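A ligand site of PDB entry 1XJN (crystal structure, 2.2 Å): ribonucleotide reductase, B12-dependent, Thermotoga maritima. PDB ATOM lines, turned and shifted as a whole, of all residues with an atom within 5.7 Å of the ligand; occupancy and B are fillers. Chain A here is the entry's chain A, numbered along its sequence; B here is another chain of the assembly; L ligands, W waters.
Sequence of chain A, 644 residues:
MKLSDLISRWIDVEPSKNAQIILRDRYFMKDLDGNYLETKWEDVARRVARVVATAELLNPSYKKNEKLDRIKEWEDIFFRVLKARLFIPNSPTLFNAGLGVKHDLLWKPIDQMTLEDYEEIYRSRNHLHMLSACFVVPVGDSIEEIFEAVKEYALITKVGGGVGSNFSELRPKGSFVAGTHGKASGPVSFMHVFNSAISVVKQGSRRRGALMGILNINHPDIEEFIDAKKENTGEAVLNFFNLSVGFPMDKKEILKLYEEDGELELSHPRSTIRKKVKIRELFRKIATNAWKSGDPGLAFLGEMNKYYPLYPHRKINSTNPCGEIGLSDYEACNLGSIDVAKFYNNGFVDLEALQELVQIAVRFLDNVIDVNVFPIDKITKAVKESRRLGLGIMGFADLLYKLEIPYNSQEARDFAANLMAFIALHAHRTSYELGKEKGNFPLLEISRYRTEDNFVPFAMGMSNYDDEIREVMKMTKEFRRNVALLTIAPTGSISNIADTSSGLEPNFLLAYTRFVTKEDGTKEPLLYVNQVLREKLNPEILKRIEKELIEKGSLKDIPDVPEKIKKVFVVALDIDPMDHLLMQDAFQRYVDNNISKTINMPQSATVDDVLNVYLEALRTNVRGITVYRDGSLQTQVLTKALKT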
ATOM      1  N   GLY A 140     -32.791   1.503   7.127  1.00  0.00           N
ATOM      2  CA  GLY A 140     -31.935   0.310   6.971  1.00  0.00           C
ATOM      3  C   GLY A 140     -30.960   0.077   8.140  1.00  0.00           C
ATOM      4  O   GLY A 140     -30.607   1.007   8.853  1.00  0.00           O
ATOM      5  N   ASP A 141     -30.550  -1.183   8.310  1.00  0.00           N
ATOM      6  CA  ASP A 141     -29.717  -1.640   9.400  1.00  0.00           C
ATOM      7  C   ASP A 141     -28.206  -1.352   9.205  1.00  0.00           C
ATOM      8  O   ASP A 141     -27.391  -2.267   9.205  1.00  0.00           O
ATOM      9  CB  ASP A 141     -29.969  -3.148   9.564  1.00  0.00           C
ATOM     10  CG  ASP A 141     -29.522  -3.674  10.857  1.00  0.00           C
ATOM     11  OD1 ASP A 141     -29.552  -2.947  11.863  1.00  0.00           O
ATOM     12  OD2 ASP A 141     -29.152  -4.880  10.885  1.00  0.00           O
ATOM     13  N   SER A 142     -27.838  -0.077   9.032  1.00  0.00           N
ATOM     14  CA  SER A 142     -26.426   0.329   8.953  1.00  0.00           C
ATOM     15  C   SER A 142     -26.345   1.763   9.426  1.00  0.00           C
ATOM     16  O   SER A 142     -27.370   2.494   9.394  1.00  0.00           O
ATOM     17  CB  SER A 142     -25.878   0.200   7.535  1.00  0.00           C
ATOM     18  OG  SER A 142     -26.518   1.164   6.719  1.00  0.00           O
ATOM     19  N   ILE A 143     -25.206   2.156   9.976  1.00  0.00           N
ATOM     20  CA  ILE A 143     -24.986   3.540  10.425  1.00  0.00           C
ATOM     21  C   ILE A 143     -25.207   4.500   9.223  1.00  0.00           C
ATOM     22  O   ILE A 143     -25.835   5.559   9.347  1.00  0.00           O
ATOM     23  CB  ILE A 143     -23.541   3.687  11.050  1.00  0.00           C
ATOM     24  CG1 ILE A 143     -23.448   2.905  12.405  1.00  0.00           C
ATOM     25  CG2 ILE A 143     -23.150   5.127  11.201  1.00  0.00           C
ATOM     26  CD1 ILE A 143     -24.366   3.434  13.587  1.00  0.00           C
ATOM     27  N   GLU A 144     -24.675   4.137   8.059  1.00  0.00           N
ATOM     28  CA  GLU A 144     -24.916   4.915   6.810  1.00  0.00           C
ATOM     29  C   GLU A 144     -26.384   5.194   6.558  1.00  0.00           C
ATOM     30  O   GLU A 144     -26.780   6.358   6.352  1.00  0.00           O
ATOM     31  CB  GLU A 144     -24.343   4.184   5.607  1.00  0.00           C
ATOM     32  CG  GLU A 144     -24.917   4.579   4.245  1.00  0.00           C
ATOM     33  CD  GLU A 144     -24.383   5.876   3.725  1.00  0.00           C
ATOM     34  OE1 GLU A 144     -23.173   6.139   3.922  1.00  0.00           O
ATOM     35  OE2 GLU A 144     -25.157   6.652   3.097  1.00  0.00           O
ATOM     36  N   ILE A 146     -29.122   4.710   8.530  1.00  0.00           N
ATOM     37  CA  ILE A 146     -29.777   5.363   9.650  1.00  0.00           C
ATOM     38  C   ILE A 146     -29.600   6.857   9.553  1.00  0.00           C
ATOM     39  O   ILE A 146     -30.535   7.615   9.749  1.00  0.00           O
ATOM     40  CB  ILE A 146     -29.223   4.901  11.017  1.00  0.00           C
ATOM     41  CG1 ILE A 146     -29.675   3.443  11.337  1.00  0.00           C
ATOM     42  CG2 ILE A 146     -29.672   5.871  12.173  1.00  0.00           C
ATOM     43  CD1 ILE A 146     -28.785   2.636  12.355  1.00  0.00           C
ATOM     44  N   LEU A 170     -33.735  -2.288  12.255  1.00  0.00           N
ATOM     45  CA  LEU A 170     -32.654  -2.115  13.187  1.00  0.00           C
ATOM     46  C   LEU A 170     -32.539  -3.290  14.144  1.00  0.00           C
ATOM     47  O   LEU A 170     -33.489  -3.595  14.909  1.00  0.00           O
ATOM     48  CB  LEU A 170     -32.729  -0.755  13.948  1.00  0.00           C
ATOM     49  CG  LEU A 170     -32.922   0.531  13.111  1.00  0.00           C
ATOM     50  CD1 LEU A 170     -32.740   1.829  13.889  1.00  0.00           C
ATOM     51  CD2 LEU A 170     -32.057   0.497  11.781  1.00  0.00           C
ATOM     52  N   ARG A 171     -31.371  -3.943  14.125  1.00  0.00           N
ATOM     53  CA  ARG A 171     -31.123  -5.109  14.995  1.00  0.00           C
ATOM     54  C   ARG A 171     -31.269  -4.707  16.447  1.00  0.00           C
ATOM     55  O   ARG A 171     -30.992  -3.551  16.773  1.00  0.00           O
ATOM     56  CB  ARG A 171     -29.754  -5.780  14.743  1.00  0.00           C
ATOM     57  CG  ARG A 171     -28.465  -4.902  15.078  1.00  0.00           C
ATOM     58  CD  ARG A 171     -27.233  -5.524  14.425  1.00  0.00           C
ATOM     59  NE  ARG A 171     -27.278  -5.458  12.950  1.00  0.00           N
ATOM     60  CZ  ARG A 171     -26.224  -5.737  12.170  1.00  0.00           C
ATOM     61  NH1 ARG A 171     -25.080  -6.085  12.720  1.00  0.00           N
ATOM     62  NH2 ARG A 171     -26.285  -5.655  10.849  1.00  0.00           N
ATOM     63  N   PHE A 176     -24.662  -8.271  18.174  1.00  0.00           N
ATOM     64  CA  PHE A 176     -23.312  -8.302  17.600  1.00  0.00           C
ATOM     65  C   PHE A 176     -23.144  -7.403  16.379  1.00  0.00           C
ATOM     66  O   PHE A 176     -23.918  -7.508  15.415  1.00  0.00           O
ATOM     67  CB  PHE A 176     -22.978  -9.783  17.260  1.00  0.00           C
ATOM     68  CG  PHE A 176     -21.784  -9.990  16.314  1.00  0.00           C
ATOM     69  CD1 PHE A 176     -21.982 -10.572  15.053  1.00  0.00           C
ATOM     70  CD2 PHE A 176     -20.477  -9.629  16.693  1.00  0.00           C
ATOM     71  CE1 PHE A 176     -20.894 -10.789  14.167  1.00  0.00           C
ATOM     72  CE2 PHE A 176     -19.371  -9.833  15.813  1.00  0.00           C
ATOM     73  CZ  PHE A 176     -19.590 -10.409  14.549  1.00  0.00           C
ATOM     74  N   VAL A 177     -22.140  -6.532  16.420  1.00  0.00           N
ATOM     75  CA  VAL A 177     -21.752  -5.680  15.274  1.00  0.00           C
ATOM     76  C   VAL A 177     -20.291  -5.959  14.863  1.00  0.00           C
ATOM     77  O   VAL A 177     -19.384  -5.862  15.706  1.00  0.00           O
ATOM     78  CB  VAL A 177     -21.879  -4.152  15.580  1.00  0.00           C
ATOM     79  CG1 VAL A 177     -21.490  -3.320  14.357  1.00  0.00           C
ATOM     80  CG2 VAL A 177     -23.259  -3.774  16.066  1.00  0.00           C
ATOM     81  N   ALA A 178     -20.052  -6.285  13.587  1.00  0.00           N
ATOM     82  CA  ALA A 178     -18.683  -6.364  13.008  1.00  0.00           C
ATOM     83  C   ALA A 178     -17.634  -5.317  13.545  1.00  0.00           C
ATOM     84  O   ALA A 178     -16.425  -5.485  13.292  1.00  0.00           O
ATOM     85  CB  ALA A 178     -18.741  -6.322  11.474  1.00  0.00           C
ATOM     86  N   GLY A 179     -18.101  -4.267  14.257  1.00  0.00           N
ATOM     87  CA  GLY A 179     -17.288  -3.344  15.109  1.00  0.00           C
ATOM     88  C   GLY A 179     -16.183  -4.019  15.943  1.00  0.00           C
ATOM     89  O   GLY A 179     -15.752  -5.102  15.559  1.00  0.00           O
ATOM     90  N   THR A 180     -15.698  -3.494  17.083  1.00  0.00           N
ATOM     91  CA  THR A 180     -16.274  -2.606  18.127  1.00  0.00           C
ATOM     92  C   THR A 180     -16.787  -3.448  19.313  1.00  0.00           C
ATOM     93  O   THR A 180     -16.016  -3.762  20.242  1.00  0.00           O
ATOM     94  CB  THR A 180     -17.212  -1.377  17.695  1.00  0.00           C
ATOM     95  OG1 THR A 180     -16.898  -0.222  18.504  1.00  0.00           O
ATOM     96  CG2 THR A 180     -18.739  -1.697  17.799  1.00  0.00           C
ATOM     97  N   GLY A 182     -18.375  -2.387  21.725  1.00  0.00           N
ATOM     98  CA  GLY A 182     -19.581  -1.727  21.211  1.00  0.00           C
ATOM     99  C   GLY A 182     -20.837  -2.565  21.437  1.00  0.00           C
ATOM    100  O   GLY A 182     -21.229  -2.810  22.590  1.00  0.00           O
ATOM    101  N   LYS A 183     -21.431  -3.035  20.327  1.00  0.00           N
ATOM    102  CA  LYS A 183     -22.762  -3.710  20.249  1.00  0.00           C
ATOM    103  C   LYS A 183     -23.939  -2.746  20.022  1.00  0.00           C
ATOM    104  O   LYS A 183     -23.959  -1.651  20.559  1.00  0.00           O
ATOM    105  CB  LYS A 183     -23.018  -4.747  21.366  1.00  0.00           C
ATOM    106  CG  LYS A 183     -22.416  -6.116  20.994  1.00  0.00           C
ATOM    107  CD  LYS A 183     -22.426  -7.106  22.136  1.00  0.00           C
ATOM    108  CE  LYS A 183     -21.309  -8.164  21.920  1.00  0.00           C
ATOM    109  NZ  LYS A 183     -21.611  -9.282  20.935  1.00  0.00           N
ATOM    110  N   ALA A 184     -24.885  -3.185  19.202  1.00  0.00           N
ATOM    111  CA  ALA A 184     -25.881  -2.332  18.576  1.00  0.00           C
ATOM    112  C   ALA A 184     -26.706  -1.573  19.580  1.00  0.00           C
ATOM    113  O   ALA A 184     -27.187  -2.150  20.552  1.00  0.00           O
ATOM    114  CB  ALA A 184     -26.784  -3.152  17.674  1.00  0.00           C
ATOM    115  N   SER A 185     -26.878  -0.271  19.381  1.00  0.00           N
ATOM    116  CA  SER A 185     -27.719   0.496  20.311  1.00  0.00           C
ATOM    117  C   SER A 185     -29.173  -0.002  20.323  1.00  0.00           C
ATOM    118  O   SER A 185     -29.844   0.096  21.340  1.00  0.00           O
ATOM    119  CB  SER A 185     -27.683   1.985  19.968  1.00  0.00           C
ATOM    120  OG  SER A 185     -26.396   2.561  20.175  1.00  0.00           O
ATOM    121  N   PHE A 190     -31.668   4.677  18.679  1.00  0.00           N
ATOM    122  CA  PHE A 190     -31.470   5.446  17.471  1.00  0.00           C
ATOM    123  C   PHE A 190     -32.647   6.400  17.253  1.00  0.00           C
ATOM    124  O   PHE A 190     -32.444   7.450  16.687  1.00  0.00           O
ATOM    125  CB  PHE A 190     -31.286   4.547  16.236  1.00  0.00           C
ATOM    126  CG  PHE A 190     -29.904   3.983  16.119  1.00  0.00           C
ATOM    127  CD1 PHE A 190     -28.795   4.820  16.040  1.00  0.00           C
ATOM    128  CD2 PHE A 190     -29.697   2.593  16.185  1.00  0.00           C
ATOM    129  CE1 PHE A 190     -27.503   4.296  16.017  1.00  0.00           C
ATOM    130  CE2 PHE A 190     -28.440   2.066  16.134  1.00  0.00           C
ATOM    131  CZ  PHE A 190     -27.333   2.925  16.048  1.00  0.00           C
ATOM    132  N   HIS B 127     -13.251  -2.009   4.997  1.00  0.00           N
ATOM    133  CA  HIS B 127     -13.834  -0.673   5.118  1.00  0.00           C
ATOM    134  C   HIS B 127     -13.590  -0.145   6.543  1.00  0.00           C
ATOM    135  O   HIS B 127     -13.680   1.035   6.813  1.00  0.00           O
ATOM    136  CB  HIS B 127     -15.355  -0.652   4.653  1.00  0.00           C
ATOM    137  CG  HIS B 127     -16.240  -1.569   5.465  1.00  0.00           C
ATOM    138  ND1 HIS B 127     -16.202  -2.946   5.346  1.00  0.00           N
ATOM    139  CD2 HIS B 127     -17.114  -1.305   6.472  1.00  0.00           C
ATOM    140  CE1 HIS B 127     -17.023  -3.490   6.237  1.00  0.00           C
ATOM    141  NE2 HIS B 127     -17.590  -2.510   6.937  1.00  0.00           N
ATOM    142  N   LYS B 158     -17.900   5.709  14.136  1.00  0.00           N
ATOM    143  CA  LYS B 158     -18.014   4.280  13.947  1.00  0.00           C
ATOM    144  C   LYS B 158     -16.653   3.613  13.725  1.00  0.00           C
ATOM    145  O   LYS B 158     -16.337   2.653  14.407  1.00  0.00           O
ATOM    146  CB  LYS B 158     -18.951   3.956  12.767  1.00  0.00           C
ATOM    147  CG  LYS B 158     -19.063   2.473  12.517  1.00  0.00           C
ATOM    148  CD  LYS B 158     -19.770   2.138  11.244  1.00  0.00           C
ATOM    149  CE  LYS B 158     -19.846   0.597  11.021  1.00  0.00           C
ATOM    150  NZ  LYS B 158     -20.198   0.336   9.592  1.00  0.00           N
ATOM    151  N   VAL B 200     -24.888   7.709  20.668  1.00  0.00           N
ATOM    152  CA  VAL B 200     -25.551   6.485  20.266  1.00  0.00           C
ATOM    153  C   VAL B 200     -24.638   5.599  19.339  1.00  0.00           C
ATOM    154  O   VAL B 200     -24.967   4.444  19.013  1.00  0.00           O
ATOM    155  CB  VAL B 200     -26.934   6.877  19.637  1.00  0.00           C
ATOM    156  CG1 VAL B 200     -27.178   6.253  18.380  1.00  0.00           C
ATOM    157  CG2 VAL B 200     -28.050   6.624  20.597  1.00  0.00           C
ATOM    158  N   VAL B 201     -23.524   6.173  18.881  1.00  0.00           N
ATOM    159  CA  VAL B 201     -22.519   5.482  18.090  1.00  0.00           C
ATOM    160  C   VAL B 201     -21.272   5.316  18.961  1.00  0.00           C
ATOM    161  O   VAL B 201     -20.580   6.284  19.250  1.00  0.00           O
ATOM    162  CB  VAL B 201     -22.106   6.225  16.732  1.00  0.00           C
ATOM    163  CG1 VAL B 201     -21.131   5.366  15.925  1.00  0.00           C
ATOM    164  CG2 VAL B 201     -23.305   6.574  15.873  1.00  0.00           C
ATOM    165  N   LYS B 202     -21.030   4.092  19.437  1.00  0.00           N
ATOM    166  CA  LYS B 202     -19.776   3.777  20.210  1.00  0.00           C
ATOM    167  C   LYS B 202     -18.545   3.773  19.266  1.00  0.00           C
ATOM    168  O   LYS B 202     -18.642   3.349  18.126  1.00  0.00           O
ATOM    169  CB  LYS B 202     -19.906   2.465  20.980  1.00  0.00           C
ATOM    170  CG  LYS B 202     -21.021   2.497  22.034  1.00  0.00           C
ATOM    171  CD  LYS B 202     -22.345   1.926  21.521  1.00  0.00           C
ATOM    172  CE  LYS B 202     -23.026   1.060  22.639  1.00  0.00           C
ATOM    173  NZ  LYS B 202     -24.337   0.393  22.235  1.00  0.00           N
ATOM    174  N   GLN B 203     -17.402   4.280  19.754  1.00  0.00           N
ATOM    175  CA  GLN B 203     -16.228   4.500  18.892  1.00  0.00           C
ATOM    176  C   GLN B 203     -15.393   3.225  18.707  1.00  0.00           C
ATOM    177  O   GLN B 203     -15.319   2.665  17.605  1.00  0.00           O
ATOM    178  CB  GLN B 203     -15.357   5.630  19.462  1.00  0.00           C
ATOM    179  CG  GLN B 203     -14.585   6.423  18.410  1.00  0.00           C
ATOM    180  CD  GLN B 203     -13.521   7.338  19.029  1.00  0.00           C
ATOM    181  OE1 GLN B 203     -12.540   6.870  19.608  1.00  0.00           O
ATOM    182  NE2 GLN B 203     -13.708   8.661  18.882  1.00  0.00           N
HETATM  183  P1  LIG L   1     -22.348  -5.460   9.686  1.00  0.00           P
HETATM  184  O1  LIG L   1     -21.228  -6.238   9.097  1.00  0.00           O
HETATM  185  O2  LIG L   1     -23.743  -5.913   9.398  1.00  0.00           O
HETATM  186  O3  LIG L   1     -22.103  -5.362  11.303  1.00  0.00           O
HETATM  187  P2  LIG L   1     -23.017  -2.860   8.190  1.00  0.00           P
HETATM  188  O4  LIG L   1     -22.107  -1.933   7.488  1.00  0.00           O
HETATM  189  O5  LIG L   1     -23.992  -3.650   7.403  1.00  0.00           O
HETATM  190  O6  LIG L   1     -22.091  -3.852   9.190  1.00  0.00           O
HETATM  191  P3  LIG L   1     -23.267  -1.245  10.463  1.00  0.00           P
HETATM  192  O7  LIG L   1     -22.943   0.083   9.929  1.00  0.00           O
HETATM  193  O8  LIG L   1     -22.257  -2.053  11.224  1.00  0.00           O
HETATM  194  O9  LIG L   1     -23.879  -2.019   9.294  1.00  0.00           O
HETATM  195  O10 LIG L   1     -24.461  -1.178  11.518  1.00  0.00           O
HETATM  196  C1  LIG L   1     -25.200  -2.304  11.844  1.00  0.00           C
HETATM  197  C2  LIG L   1     -26.207  -2.011  12.955  1.00  0.00           C
HETATM  198  O11 LIG L   1     -25.525  -1.925  14.209  1.00  0.00           O
HETATM  199  C3  LIG L   1     -27.042  -0.725  12.853  1.00  0.00           C
HETATM  200  O12 LIG L   1     -28.338  -0.962  13.440  1.00  0.00           O
HETATM  201  C4  LIG L   1     -26.230   0.236  13.722  1.00  0.00           C
HETATM  202  C5  LIG L   1     -25.564  -0.647  14.734  1.00  0.00           C
HETATM  203  N1  LIG L   1     -24.166  -0.161  14.936  1.00  0.00           N
HETATM  204  C6  LIG L   1     -23.124  -0.313  14.115  1.00  0.00           C
HETATM  205  N2  LIG L   1     -22.054   0.254  14.652  1.00  0.00           N
HETATM  206  C7  LIG L   1     -22.407   0.789  15.809  1.00  0.00           C
HETATM  207  C8  LIG L   1     -21.707   1.497  16.776  1.00  0.00           C
HETATM  208  N3  LIG L   1     -20.394   1.773  16.592  1.00  0.00           N
HETATM  209  N4  LIG L   1     -22.374   1.883  17.876  1.00  0.00           N
HETATM  210  C9  LIG L   1     -23.643   1.596  18.056  1.00  0.00           C
HETATM  211  N5  LIG L   1     -24.329   0.936  17.132  1.00  0.00           N
HETATM  212  C10 LIG L   1     -23.733   0.496  16.018  1.00  0.00           C
HETATM  213  O   HOH W   1     -26.357  -4.338   7.869  1.00  0.00           O
HETATM  214  O   HOH W   2     -29.335  -1.266  16.225  1.00  0.00           O
HETATM  215  O   HOH W   3     -22.698   1.932   7.582  1.00  0.00           O
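The backbone carbonyl oxygen (O) of Phe 176 sits at hydrogen-bond distance from the guanidinium group (NH1) of Arg 171 (3.3 Å). The backbone carbonyl oxygen (O) of Lys 183 is in hydrogen-bond range of the side-chain amino group (NZ) of Lys 202 of chain B, at 2.7 Å. OD2 of Asp 141 lies within salt-bridge range of NE of Arg 171 (2.8 Å). O of Val 200 of chain B sits at hydrogen-bond distance from OG of Ser 185 (2.6 Å).
Water W1 lies within hydrogen-bond range of an oxygen (O5) of the ligand, the backbone carbonyl oxygen of Asp 141 and the guanidinium group of Arg 171. Water W2 lies within hydrogen-bond range of O of Arg 171 (2.9 Å) and O12 of the ligand (3.0 Å). Water W3 lies within hydrogen-bond range of an oxygen (O7) of the ligand (3.0 Å), the backbone NH of Glu 144 (3.0 Å) and the backbone NH of Ile 143 (3.5 Å).
O3 of the ligand lies within hydrogen-bond range of N of Ala 178 (3.2 Å). The backbone NH (N) of Ile 143 sits at hydrogen-bond distance from an oxygen (O7) of the ligand, 3.1 Å away. The backbone carbonyl oxygen (O) of Lys 202 of chain B lies within hydrogen-bond range of a nitrogen (N3) of the ligand (2.8 Å). An oxygen (O7) of the ligand lies within salt-bridge range of the side-chain amino group (NZ) of Lys 158 of chain B (2.8 Å). N4 of the ligand is in hydrogen-bond range of N of Lys 202 of chain B, at 3.0 Å. O2 of the ligand lies within salt-bridge range of NH2 of Arg 171. An oxygen (O12) of the ligand is in hydrogen-bond range of the side-chain carboxylate (OD1) of Asp 141 (2.8 Å).
Residues that only touch the ligand: Val 200 of chain B (3.3 Å), Val 177 (3.4 Å), Ser 142 (3.5 Å), Ser 185 (3.6 Å), Val 201 of chain B (3.6 Å), Phe 190 (3.7 Å), Ile 146 (3.8 Å) and Ala 184 (3.9 Å). Hydrophobic or aromatic side chains that line the ligand: Ile 143, Ile 146, Val 177, Ala 178, Ala 184, Phe 190 and Val 201 of chain B. The nearest printed residue that does not touch the ligand is Thr 180 (4.03 Å).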
